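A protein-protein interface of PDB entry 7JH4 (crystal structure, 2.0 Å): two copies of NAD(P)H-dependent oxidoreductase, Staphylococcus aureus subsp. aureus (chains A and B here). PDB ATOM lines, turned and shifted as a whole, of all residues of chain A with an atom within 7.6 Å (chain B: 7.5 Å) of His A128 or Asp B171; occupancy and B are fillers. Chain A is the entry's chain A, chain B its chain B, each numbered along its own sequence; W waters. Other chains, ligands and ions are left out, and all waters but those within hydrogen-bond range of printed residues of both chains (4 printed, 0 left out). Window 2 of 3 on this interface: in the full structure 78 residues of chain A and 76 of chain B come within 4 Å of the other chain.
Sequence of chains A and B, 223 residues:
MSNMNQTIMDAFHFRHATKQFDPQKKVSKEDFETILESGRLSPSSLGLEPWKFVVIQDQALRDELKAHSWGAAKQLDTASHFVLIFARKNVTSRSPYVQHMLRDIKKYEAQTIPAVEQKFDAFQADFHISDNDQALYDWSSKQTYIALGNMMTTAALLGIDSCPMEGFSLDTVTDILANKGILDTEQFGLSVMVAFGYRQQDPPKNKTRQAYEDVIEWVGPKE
The side-chain carboxylate (OD2) of Asp A126 is in hydrogen-bond range of the side-chain hydroxyl (OG) of Ser B169, 2.8 Å away.
O of Asp A126 is in hydrogen-bond range of N of Leu B170 (3.4 Å).
The side-chain carboxylate of Asp B171 sits at hydrogen-bond distance from a ring nitrogen (NE2) of His A128, at 2.7 Å.
The side-chain amide nitrogen of Asn A132 sits at hydrogen-bond distance from the side-chain amide oxygen of Gln B134.
N of Ala A135 lies close to NE2 of Gln B134 (3.2 Å).
ND1 of His A128 lies within hydrogen-bond range of OD2 of Asp A131 (2.8 Å).
The side-chain amide oxygen (OD1) of Asn A132 lies close to the backbone NH (N) of Gln A134 (3.3 Å).
The side-chain amide oxygen (OD1) of Asn A132 is in hydrogen-bond range of the backbone NH (N) of Ala A135.
The backbone carbonyl oxygen (O) of Leu B170 sits at hydrogen-bond distance from the side-chain hydroxyl (OG1) of Thr B174 (2.9 Å).
Among the printed residues, merely in contact across the chains: Phe A127 with Phe B168, Phe A127 with Leu B170 and Gln A134 with Gln B134.
Of chain B, only Asp B171 comes within 4 Å of His A128.
Of the printed residues of chain A, Asp B171 touches His A128.
Of the printed residues of chain B, Ala A135 touches Gln B134 (3.2 Å).
Of the printed residues of chain B, Phe A127 touches Phe B168 and Leu B170.
Printed residues of chain B within 4 Å of Asp A126: Ser B169 and Leu B170.
Of the printed residues of chain A, Ser B169 touches Asp A126 (2.8 Å).
Ala A122 touches none of the printed residues of chain B.
Phe A123 touches none of the printed residues of chain B.
The nearest residue of chain A that does not touch Asp B171 is Asp A126 (4.8 Å).
Of the 15 printed residues of chain A, 6 touch a printed residue of chain B.
Of the 12 printed residues of chain B, 5 touch a printed residue of chain A.
Hydrophobic or aromatic side chains of chain B within 4 Å of the printed part of chain A: Phe B168 and Leu B170.
Along chain B the printed residues that touch a printed residue of chain A span positions 134 to 171.
Gln A134 touches its own counterpart, Gln B134.
1 position is printed for both chains.
Water W2 lies within hydrogen-bond range of the backbone carbonyl oxygen of Ala A135 (2.7 Å), the side-chain carboxylate of Asp B138 (3.1 Å) and the backbone NH of Trp A139 (3.1 Å).
Water W3 lies within hydrogen-bond range of the side-chain carboxylate (OD2) of Asp B138, the side-chain amide nitrogen (NE2) of Gln B134 and the side-chain amide nitrogen (NE2) of Gln A134.
Water W1 bridges the backbone carbonyl oxygen of Asp A126 (2.9 Å) and the side-chain carboxylate of Asp B171 (3.1 Å).
Water W4 lies within hydrogen-bond range of the backbone carbonyl oxygen (O) of Phe B168 and the side-chain carboxylate (OD2) of Asp A126.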
ATOM      1  N   ALA A 122     -12.549  -4.830 -37.860  1.00  0.00           N
ATOM      2  CA  ALA A 122     -11.222  -5.096 -37.312  1.00  0.00           C
ATOM      3  C   ALA A 122     -11.183  -4.845 -35.816  1.00  0.00           C
ATOM      4  O   ALA A 122     -10.600  -5.636 -35.065  1.00  0.00           O
ATOM      5  CB  ALA A 122     -10.172  -4.236 -38.021  1.00  0.00           C
ATOM      6  N   PHE A 123     -11.787  -3.746 -35.361  1.00  0.00           N
ATOM      7  CA  PHE A 123     -11.923  -3.531 -33.926  1.00  0.00           C
ATOM      8  C   PHE A 123     -12.613  -4.721 -33.258  1.00  0.00           C
ATOM      9  O   PHE A 123     -12.133  -5.243 -32.246  1.00  0.00           O
ATOM     10  CB  PHE A 123     -12.688  -2.233 -33.653  1.00  0.00           C
ATOM     11  CG  PHE A 123     -13.332  -2.179 -32.282  1.00  0.00           C
ATOM     12  CD1 PHE A 123     -12.552  -2.196 -31.124  1.00  0.00           C
ATOM     13  CD2 PHE A 123     -14.713  -2.104 -32.152  1.00  0.00           C
ATOM     14  CE1 PHE A 123     -13.136  -2.137 -29.866  1.00  0.00           C
ATOM     15  CE2 PHE A 123     -15.313  -2.036 -30.888  1.00  0.00           C
ATOM     16  CZ  PHE A 123     -14.525  -2.060 -29.741  1.00  0.00           C
ATOM     17  N   GLN A 124     -13.733  -5.182 -33.821  1.00  0.00           N
ATOM     18  CA  GLN A 124     -14.456  -6.275 -33.170  1.00  0.00           C
ATOM     19  C   GLN A 124     -13.593  -7.530 -33.065  1.00  0.00           C
ATOM     20  O   GLN A 124     -13.604  -8.217 -32.037  1.00  0.00           O
ATOM     21  CB  GLN A 124     -15.767  -6.550 -33.915  1.00  0.00           C
ATOM     22  CG  GLN A 124     -16.791  -5.473 -33.647  1.00  0.00           C
ATOM     23  CD  GLN A 124     -18.194  -5.814 -34.103  1.00  0.00           C
ATOM     24  OE1 GLN A 124     -18.401  -6.493 -35.116  1.00  0.00           O
ATOM     25  NE2 GLN A 124     -19.178  -5.337 -33.348  1.00  0.00           N
ATOM     26  N   ALA A 125     -12.819  -7.834 -34.106  1.00  0.00           N
ATOM     27  CA  ALA A 125     -11.888  -8.951 -34.003  1.00  0.00           C
ATOM     28  C   ALA A 125     -10.779  -8.656 -33.001  1.00  0.00           C
ATOM     29  O   ALA A 125     -10.399  -9.529 -32.212  1.00  0.00           O
ATOM     30  CB  ALA A 125     -11.297  -9.277 -35.374  1.00  0.00           C
ATOM     31  N   ASP A 126     -10.241  -7.436 -33.019  1.00  0.00           N
ATOM     32  CA  ASP A 126      -9.117  -7.104 -32.150  1.00  0.00           C
ATOM     33  C   ASP A 126      -9.505  -7.123 -30.676  1.00  0.00           C
ATOM     34  O   ASP A 126      -8.631  -7.254 -29.814  1.00  0.00           O
ATOM     35  CB  ASP A 126      -8.564  -5.728 -32.533  1.00  0.00           C
ATOM     36  CG  ASP A 126      -7.115  -5.547 -32.152  1.00  0.00           C
ATOM     37  OD1 ASP A 126      -6.344  -6.531 -32.214  1.00  0.00           O
ATOM     38  OD2 ASP A 126      -6.742  -4.407 -31.802  1.00  0.00           O
ATOM     39  N   PHE A 127     -10.793  -6.974 -30.382  1.00  0.00           N
ATOM     40  CA  PHE A 127     -11.326  -7.011 -29.031  1.00  0.00           C
ATOM     41  C   PHE A 127     -12.078  -8.309 -28.747  1.00  0.00           C
ATOM     42  O   PHE A 127     -12.695  -8.431 -27.688  1.00  0.00           O
ATOM     43  CB  PHE A 127     -12.248  -5.806 -28.805  1.00  0.00           C
ATOM     44  CG  PHE A 127     -12.285  -5.323 -27.382  1.00  0.00           C
ATOM     45  CD1 PHE A 127     -11.172  -4.739 -26.803  1.00  0.00           C
ATOM     46  CD2 PHE A 127     -13.442  -5.442 -26.629  1.00  0.00           C
ATOM     47  CE1 PHE A 127     -11.214  -4.295 -25.489  1.00  0.00           C
ATOM     48  CE2 PHE A 127     -13.486  -4.998 -25.317  1.00  0.00           C
ATOM     49  CZ  PHE A 127     -12.382  -4.420 -24.752  1.00  0.00           C
ATOM     50  N   HIS A 128     -12.070  -9.260 -29.685  1.00  0.00           N
ATOM     51  CA  HIS A 128     -12.699 -10.569 -29.538  1.00  0.00           C
ATOM     52  C   HIS A 128     -14.217 -10.485 -29.431  1.00  0.00           C
ATOM     53  O   HIS A 128     -14.866 -11.465 -29.037  1.00  0.00           O
ATOM     54  CB  HIS A 128     -12.122 -11.326 -28.336  1.00  0.00           C
ATOM     55  CG  HIS A 128     -10.700 -11.752 -28.528  1.00  0.00           C
ATOM     56  ND1 HIS A 128     -10.342 -12.813 -29.333  1.00  0.00           N
ATOM     57  CD2 HIS A 128      -9.544 -11.255 -28.028  1.00  0.00           C
ATOM     58  CE1 HIS A 128      -9.028 -12.947 -29.325  1.00  0.00           C
ATOM     59  NE2 HIS A 128      -8.519 -12.013 -28.541  1.00  0.00           N
ATOM     60  N   ILE A 129     -14.792  -9.335 -29.782  1.00  0.00           N
ATOM     61  CA  ILE A 129     -16.243  -9.173 -29.761  1.00  0.00           C
ATOM     62  C   ILE A 129     -16.909 -10.106 -30.765  1.00  0.00           C
ATOM     63  O   ILE A 129     -17.990 -10.645 -30.508  1.00  0.00           O
ATOM     64  CB  ILE A 129     -16.606  -7.699 -30.039  1.00  0.00           C
ATOM     65  CG1 ILE A 129     -16.180  -6.809 -28.877  1.00  0.00           C
ATOM     66  CG2 ILE A 129     -18.091  -7.562 -30.354  1.00  0.00           C
ATOM     67  CD1 ILE A 129     -16.061  -5.314 -29.262  1.00  0.00           C
ATOM     68  N   SER A 130     -16.290 -10.301 -31.931  1.00  0.00           N
ATOM     69  CA  SER A 130     -16.913 -11.057 -33.009  1.00  0.00           C
ATOM     70  C   SER A 130     -16.464 -12.517 -33.041  1.00  0.00           C
ATOM     71  O   SER A 130     -16.682 -13.205 -34.045  1.00  0.00           O
ATOM     72  CB  SER A 130     -16.641 -10.384 -34.359  1.00  0.00           C
ATOM     73  OG  SER A 130     -15.255 -10.183 -34.557  1.00  0.00           O
ATOM     74  N   ASP A 131     -15.858 -13.010 -31.957  1.00  0.00           N
ATOM     75  CA  ASP A 131     -15.492 -14.422 -31.909  1.00  0.00           C
ATOM     76  C   ASP A 131     -16.716 -15.325 -32.016  1.00  0.00           C
ATOM     77  O   ASP A 131     -16.642 -16.410 -32.604  1.00  0.00           O
ATOM     78  CB  ASP A 131     -14.730 -14.747 -30.623  1.00  0.00           C
ATOM     79  CG  ASP A 131     -13.361 -14.104 -30.570  1.00  0.00           C
ATOM     80  OD1 ASP A 131     -13.059 -13.244 -31.424  1.00  0.00           O
ATOM     81  OD2 ASP A 131     -12.591 -14.453 -29.654  1.00  0.00           O
ATOM     82  N   ASN A 132     -17.841 -14.923 -31.430  1.00  0.00           N
ATOM     83  CA  ASN A 132     -19.035 -15.763 -31.460  1.00  0.00           C
ATOM     84  C   ASN A 132     -20.228 -14.904 -31.082  1.00  0.00           C
ATOM     85  O   ASN A 132     -20.073 -13.768 -30.633  1.00  0.00           O
ATOM     86  CB  ASN A 132     -18.909 -16.982 -30.529  1.00  0.00           C
ATOM     87  CG  ASN A 132     -18.499 -16.601 -29.108  1.00  0.00           C
ATOM     88  OD1 ASN A 132     -19.269 -15.978 -28.359  1.00  0.00           O
ATOM     89  ND2 ASN A 132     -17.285 -16.985 -28.729  1.00  0.00           N
ATOM     90  N   GLN A 134     -22.406 -15.123 -28.713  1.00  0.00           N
ATOM     91  CA  GLN A 134     -22.530 -14.808 -27.298  1.00  0.00           C
ATOM     92  C   GLN A 134     -21.651 -13.614 -26.941  1.00  0.00           C
ATOM     93  O   GLN A 134     -22.092 -12.682 -26.254  1.00  0.00           O
ATOM     94  CB  GLN A 134     -22.167 -16.046 -26.473  1.00  0.00           C
ATOM     95  CG  GLN A 134     -22.161 -15.847 -24.962  1.00  0.00           C
ATOM     96  CD  GLN A 134     -21.569 -17.037 -24.218  1.00  0.00           C
ATOM     97  OE1 GLN A 134     -21.986 -18.173 -24.423  1.00  0.00           O
ATOM     98  NE2 GLN A 134     -20.588 -16.782 -23.366  1.00  0.00           N
ATOM     99  N   ALA A 135     -20.400 -13.618 -27.415  1.00  0.00           N
ATOM    100  CA  ALA A 135     -19.516 -12.484 -27.169  1.00  0.00           C
ATOM    101  C   ALA A 135     -20.069 -11.220 -27.806  1.00  0.00           C
ATOM    102  O   ALA A 135     -19.986 -10.133 -27.224  1.00  0.00           O
ATOM    103  CB  ALA A 135     -18.120 -12.762 -27.713  1.00  0.00           C
ATOM    104  N   LEU A 136     -20.625 -11.345 -29.011  1.00  0.00           N
ATOM    105  CA  LEU A 136     -21.143 -10.175 -29.705  1.00  0.00           C
ATOM    106  C   LEU A 136     -22.356  -9.621 -28.976  1.00  0.00           C
ATOM    107  O   LEU A 136     -22.501  -8.405 -28.827  1.00  0.00           O
ATOM    108  CB  LEU A 136     -21.478 -10.545 -31.153  1.00  0.00           C
ATOM    109  CG  LEU A 136     -22.061  -9.526 -32.130  1.00  0.00           C
ATOM    110  CD1 LEU A 136     -21.143  -8.309 -32.261  1.00  0.00           C
ATOM    111  CD2 LEU A 136     -22.240 -10.184 -33.480  1.00  0.00           C
ATOM    112  N   TRP A 139     -21.271  -8.036 -25.543  1.00  0.00           N
ATOM    113  CA  TRP A 139     -20.659  -6.721 -25.730  1.00  0.00           C
ATOM    114  C   TRP A 139     -21.720  -5.616 -25.770  1.00  0.00           C
ATOM    115  O   TRP A 139     -21.602  -4.611 -25.062  1.00  0.00           O
ATOM    116  CB  TRP A 139     -19.800  -6.726 -27.001  1.00  0.00           C
ATOM    117  CG  TRP A 139     -19.319  -5.372 -27.470  1.00  0.00           C
ATOM    118  CD1 TRP A 139     -18.410  -4.541 -26.843  1.00  0.00           C
ATOM    119  CD2 TRP A 139     -19.703  -4.705 -28.675  1.00  0.00           C
ATOM    120  NE1 TRP A 139     -18.225  -3.399 -27.592  1.00  0.00           N
ATOM    121  CE2 TRP A 139     -19.009  -3.476 -28.717  1.00  0.00           C
ATOM    122  CE3 TRP A 139     -20.577  -5.026 -29.726  1.00  0.00           C
ATOM    123  CZ2 TRP A 139     -19.149  -2.573 -29.776  1.00  0.00           C
ATOM    124  CZ3 TRP A 139     -20.720  -4.121 -30.773  1.00  0.00           C
ATOM    125  CH2 TRP A 139     -20.007  -2.910 -30.785  1.00  0.00           C
ATOM    126  N   GLN B 134     -16.230 -17.822 -20.765  1.00  0.00           N
ATOM    127  CA  GLN B 134     -16.418 -16.545 -21.436  1.00  0.00           C
ATOM    128  C   GLN B 134     -17.605 -15.802 -20.840  1.00  0.00           C
ATOM    129  O   GLN B 134     -17.507 -14.616 -20.490  1.00  0.00           O
ATOM    130  CB  GLN B 134     -16.612 -16.781 -22.937  1.00  0.00           C
ATOM    131  CG  GLN B 134     -16.786 -15.516 -23.773  1.00  0.00           C
ATOM    132  CD  GLN B 134     -17.210 -15.820 -25.201  1.00  0.00           C
ATOM    133  OE1 GLN B 134     -16.547 -16.581 -25.921  1.00  0.00           O
ATOM    134  NE2 GLN B 134     -18.328 -15.234 -25.619  1.00  0.00           N
ATOM    135  N   ASP B 138     -17.504 -12.250 -18.843  1.00  0.00           N
ATOM    136  CA  ASP B 138     -18.205 -11.092 -19.405  1.00  0.00           C
ATOM    137  C   ASP B 138     -19.308 -10.613 -18.481  1.00  0.00           C
ATOM    138  O   ASP B 138     -19.656  -9.428 -18.497  1.00  0.00           O
ATOM    139  CB  ASP B 138     -18.789 -11.416 -20.784  1.00  0.00           C
ATOM    140  CG  ASP B 138     -17.776 -11.252 -21.905  1.00  0.00           C
ATOM    141  OD1 ASP B 138     -16.761 -10.540 -21.730  1.00  0.00           O
ATOM    142  OD2 ASP B 138     -18.017 -11.826 -22.987  1.00  0.00           O
ATOM    143  N   PHE B 168      -8.484  -0.823 -27.949  1.00  0.00           N
ATOM    144  CA  PHE B 168      -7.121  -1.292 -27.751  1.00  0.00           C
ATOM    145  C   PHE B 168      -7.045  -2.775 -28.078  1.00  0.00           C
ATOM    146  O   PHE B 168      -8.052  -3.485 -28.087  1.00  0.00           O
ATOM    147  CB  PHE B 168      -6.622  -1.025 -26.316  1.00  0.00           C
ATOM    148  CG  PHE B 168      -7.530  -1.583 -25.240  1.00  0.00           C
ATOM    149  CD1 PHE B 168      -8.623  -0.850 -24.784  1.00  0.00           C
ATOM    150  CD2 PHE B 168      -7.291  -2.837 -24.687  1.00  0.00           C
ATOM    151  CE1 PHE B 168      -9.460  -1.359 -23.792  1.00  0.00           C
ATOM    152  CE2 PHE B 168      -8.114  -3.354 -23.700  1.00  0.00           C
ATOM    153  CZ  PHE B 168      -9.211  -2.616 -23.253  1.00  0.00           C
ATOM    154  N   SER B 169      -5.833  -3.225 -28.375  1.00  0.00           N
ATOM    155  CA  SER B 169      -5.577  -4.606 -28.770  1.00  0.00           C
ATOM    156  C   SER B 169      -5.599  -5.452 -27.507  1.00  0.00           C
ATOM    157  O   SER B 169      -4.621  -5.498 -26.752  1.00  0.00           O
ATOM    158  CB  SER B 169      -4.245  -4.709 -29.499  1.00  0.00           C
ATOM    159  OG  SER B 169      -4.256  -3.867 -30.641  1.00  0.00           O
ATOM    160  N   LEU B 170      -6.736  -6.099 -27.257  1.00  0.00           N
ATOM    161  CA  LEU B 170      -6.948  -6.771 -25.979  1.00  0.00           C
ATOM    162  C   LEU B 170      -5.762  -7.673 -25.624  1.00  0.00           C
ATOM    163  O   LEU B 170      -5.127  -7.497 -24.580  1.00  0.00           O
ATOM    164  CB  LEU B 170      -8.258  -7.562 -26.023  1.00  0.00           C
ATOM    165  CG  LEU B 170      -8.783  -8.140 -24.700  1.00  0.00           C
ATOM    166  CD1 LEU B 170      -8.583  -7.130 -23.566  1.00  0.00           C
ATOM    167  CD2 LEU B 170     -10.243  -8.536 -24.815  1.00  0.00           C
ATOM    168  N   ASP B 171      -5.444  -8.644 -26.485  1.00  0.00           N
ATOM    169  CA  ASP B 171      -4.417  -9.632 -26.131  1.00  0.00           C
ATOM    170  C   ASP B 171      -3.057  -8.990 -25.913  1.00  0.00           C
ATOM    171  O   ASP B 171      -2.330  -9.370 -24.987  1.00  0.00           O
ATOM    172  CB  ASP B 171      -4.308 -10.713 -27.202  1.00  0.00           C
ATOM    173  CG  ASP B 171      -5.586 -11.496 -27.350  1.00  0.00           C
ATOM    174  OD1 ASP B 171      -6.355 -11.578 -26.369  1.00  0.00           O
ATOM    175  OD2 ASP B 171      -5.835 -12.016 -28.450  1.00  0.00           O
ATOM    176  N   THR B 172      -2.680  -8.031 -26.766  1.00  0.00           N
ATOM    177  CA  THR B 172      -1.351  -7.445 -26.642  1.00  0.00           C
ATOM    178  C   THR B 172      -1.235  -6.580 -25.395  1.00  0.00           C
ATOM    179  O   THR B 172      -0.212  -6.622 -24.703  1.00  0.00           O
ATOM    180  CB  THR B 172      -1.009  -6.627 -27.886  1.00  0.00           C
ATOM    181  OG1 THR B 172      -0.946  -7.495 -29.025  1.00  0.00           O
ATOM    182  CG2 THR B 172       0.341  -5.937 -27.688  1.00  0.00           C
ATOM    183  N   VAL B 173      -2.260  -5.782 -25.090  1.00  0.00           N
ATOM    184  CA  VAL B 173      -2.186  -4.947 -23.894  1.00  0.00           C
ATOM    185  C   VAL B 173      -2.225  -5.808 -22.637  1.00  0.00           C
ATOM    186  O   VAL B 173      -1.626  -5.453 -21.611  1.00  0.00           O
ATOM    187  CB  VAL B 173      -3.318  -3.899 -23.900  1.00  0.00           C
ATOM    188  CG1 VAL B 173      -3.362  -3.164 -22.573  1.00  0.00           C
ATOM    189  CG2 VAL B 173      -3.111  -2.910 -25.049  1.00  0.00           C
ATOM    190  N   THR B 174      -2.929  -6.941 -22.690  1.00  0.00           N
ATOM    191  CA  THR B 174      -2.993  -7.821 -21.529  1.00  0.00           C
ATOM    192  C   THR B 174      -1.617  -8.389 -21.204  1.00  0.00           C
ATOM    193  O   THR B 174      -1.243  -8.490 -20.027  1.00  0.00           O
ATOM    194  CB  THR B 174      -4.002  -8.947 -21.777  1.00  0.00           C
ATOM    195  OG1 THR B 174      -5.337  -8.410 -21.785  1.00  0.00           O
ATOM    196  CG2 THR B 174      -3.895 -10.012 -20.695  1.00  0.00           C
ATOM    197  N   ASP B 175      -0.846  -8.759 -22.234  1.00  0.00           N
ATOM    198  CA  ASP B 175       0.481  -9.328 -21.993  1.00  0.00           C
ATOM    199  C   ASP B 175       1.438  -8.274 -21.456  1.00  0.00           C
ATOM    200  O   ASP B 175       2.260  -8.563 -20.576  1.00  0.00           O
ATOM    201  CB  ASP B 175       1.036  -9.951 -23.274  1.00  0.00           C
ATOM    202  CG  ASP B 175       0.191 -11.114 -23.767  1.00  0.00           C
ATOM    203  OD1 ASP B 175      -0.536 -11.712 -22.943  1.00  0.00           O
ATOM    204  OD2 ASP B 175       0.235 -11.426 -24.977  1.00  0.00           O
ATOM    205  N   ILE B 176       1.354  -7.049 -21.975  1.00  0.00           N
ATOM    206  CA  ILE B 176       2.197  -5.974 -21.465  1.00  0.00           C
ATOM    207  C   ILE B 176       1.940  -5.777 -19.975  1.00  0.00           C
ATOM    208  O   ILE B 176       2.856  -5.866 -19.148  1.00  0.00           O
ATOM    209  CB  ILE B 176       1.971  -4.681 -22.268  1.00  0.00           C
ATOM    210  CG1 ILE B 176       2.424  -4.886 -23.724  1.00  0.00           C
ATOM    211  CG2 ILE B 176       2.731  -3.515 -21.642  1.00  0.00           C
ATOM    212  CD1 ILE B 176       2.222  -3.674 -24.614  1.00  0.00           C
ATOM    213  N   LEU B 177       0.677  -5.552 -19.605  1.00  0.00           N
ATOM    214  CA  LEU B 177       0.349  -5.376 -18.194  1.00  0.00           C
ATOM    215  C   LEU B 177       0.721  -6.612 -17.379  1.00  0.00           C
ATOM    216  O   LEU B 177       1.204  -6.492 -16.246  1.00  0.00           O
ATOM    217  CB  LEU B 177      -1.137  -5.062 -18.038  1.00  0.00           C
ATOM    218  CG  LEU B 177      -1.594  -3.732 -18.632  1.00  0.00           C
ATOM    219  CD1 LEU B 177      -3.133  -3.676 -18.647  1.00  0.00           C
ATOM    220  CD2 LEU B 177      -1.012  -2.590 -17.835  1.00  0.00           C
HETATM  221  O   HOH W   1      -6.482  -9.162 -29.352  1.00  0.00           O
HETATM  222  O   HOH W   2     -18.619  -9.585 -25.015  1.00  0.00           O
HETATM  223  O   HOH W   3     -19.777 -13.777 -23.565  1.00  0.00           O
HETATM  224  O   HOH W   4      -9.273  -2.537 -30.783  1.00  0.00           O
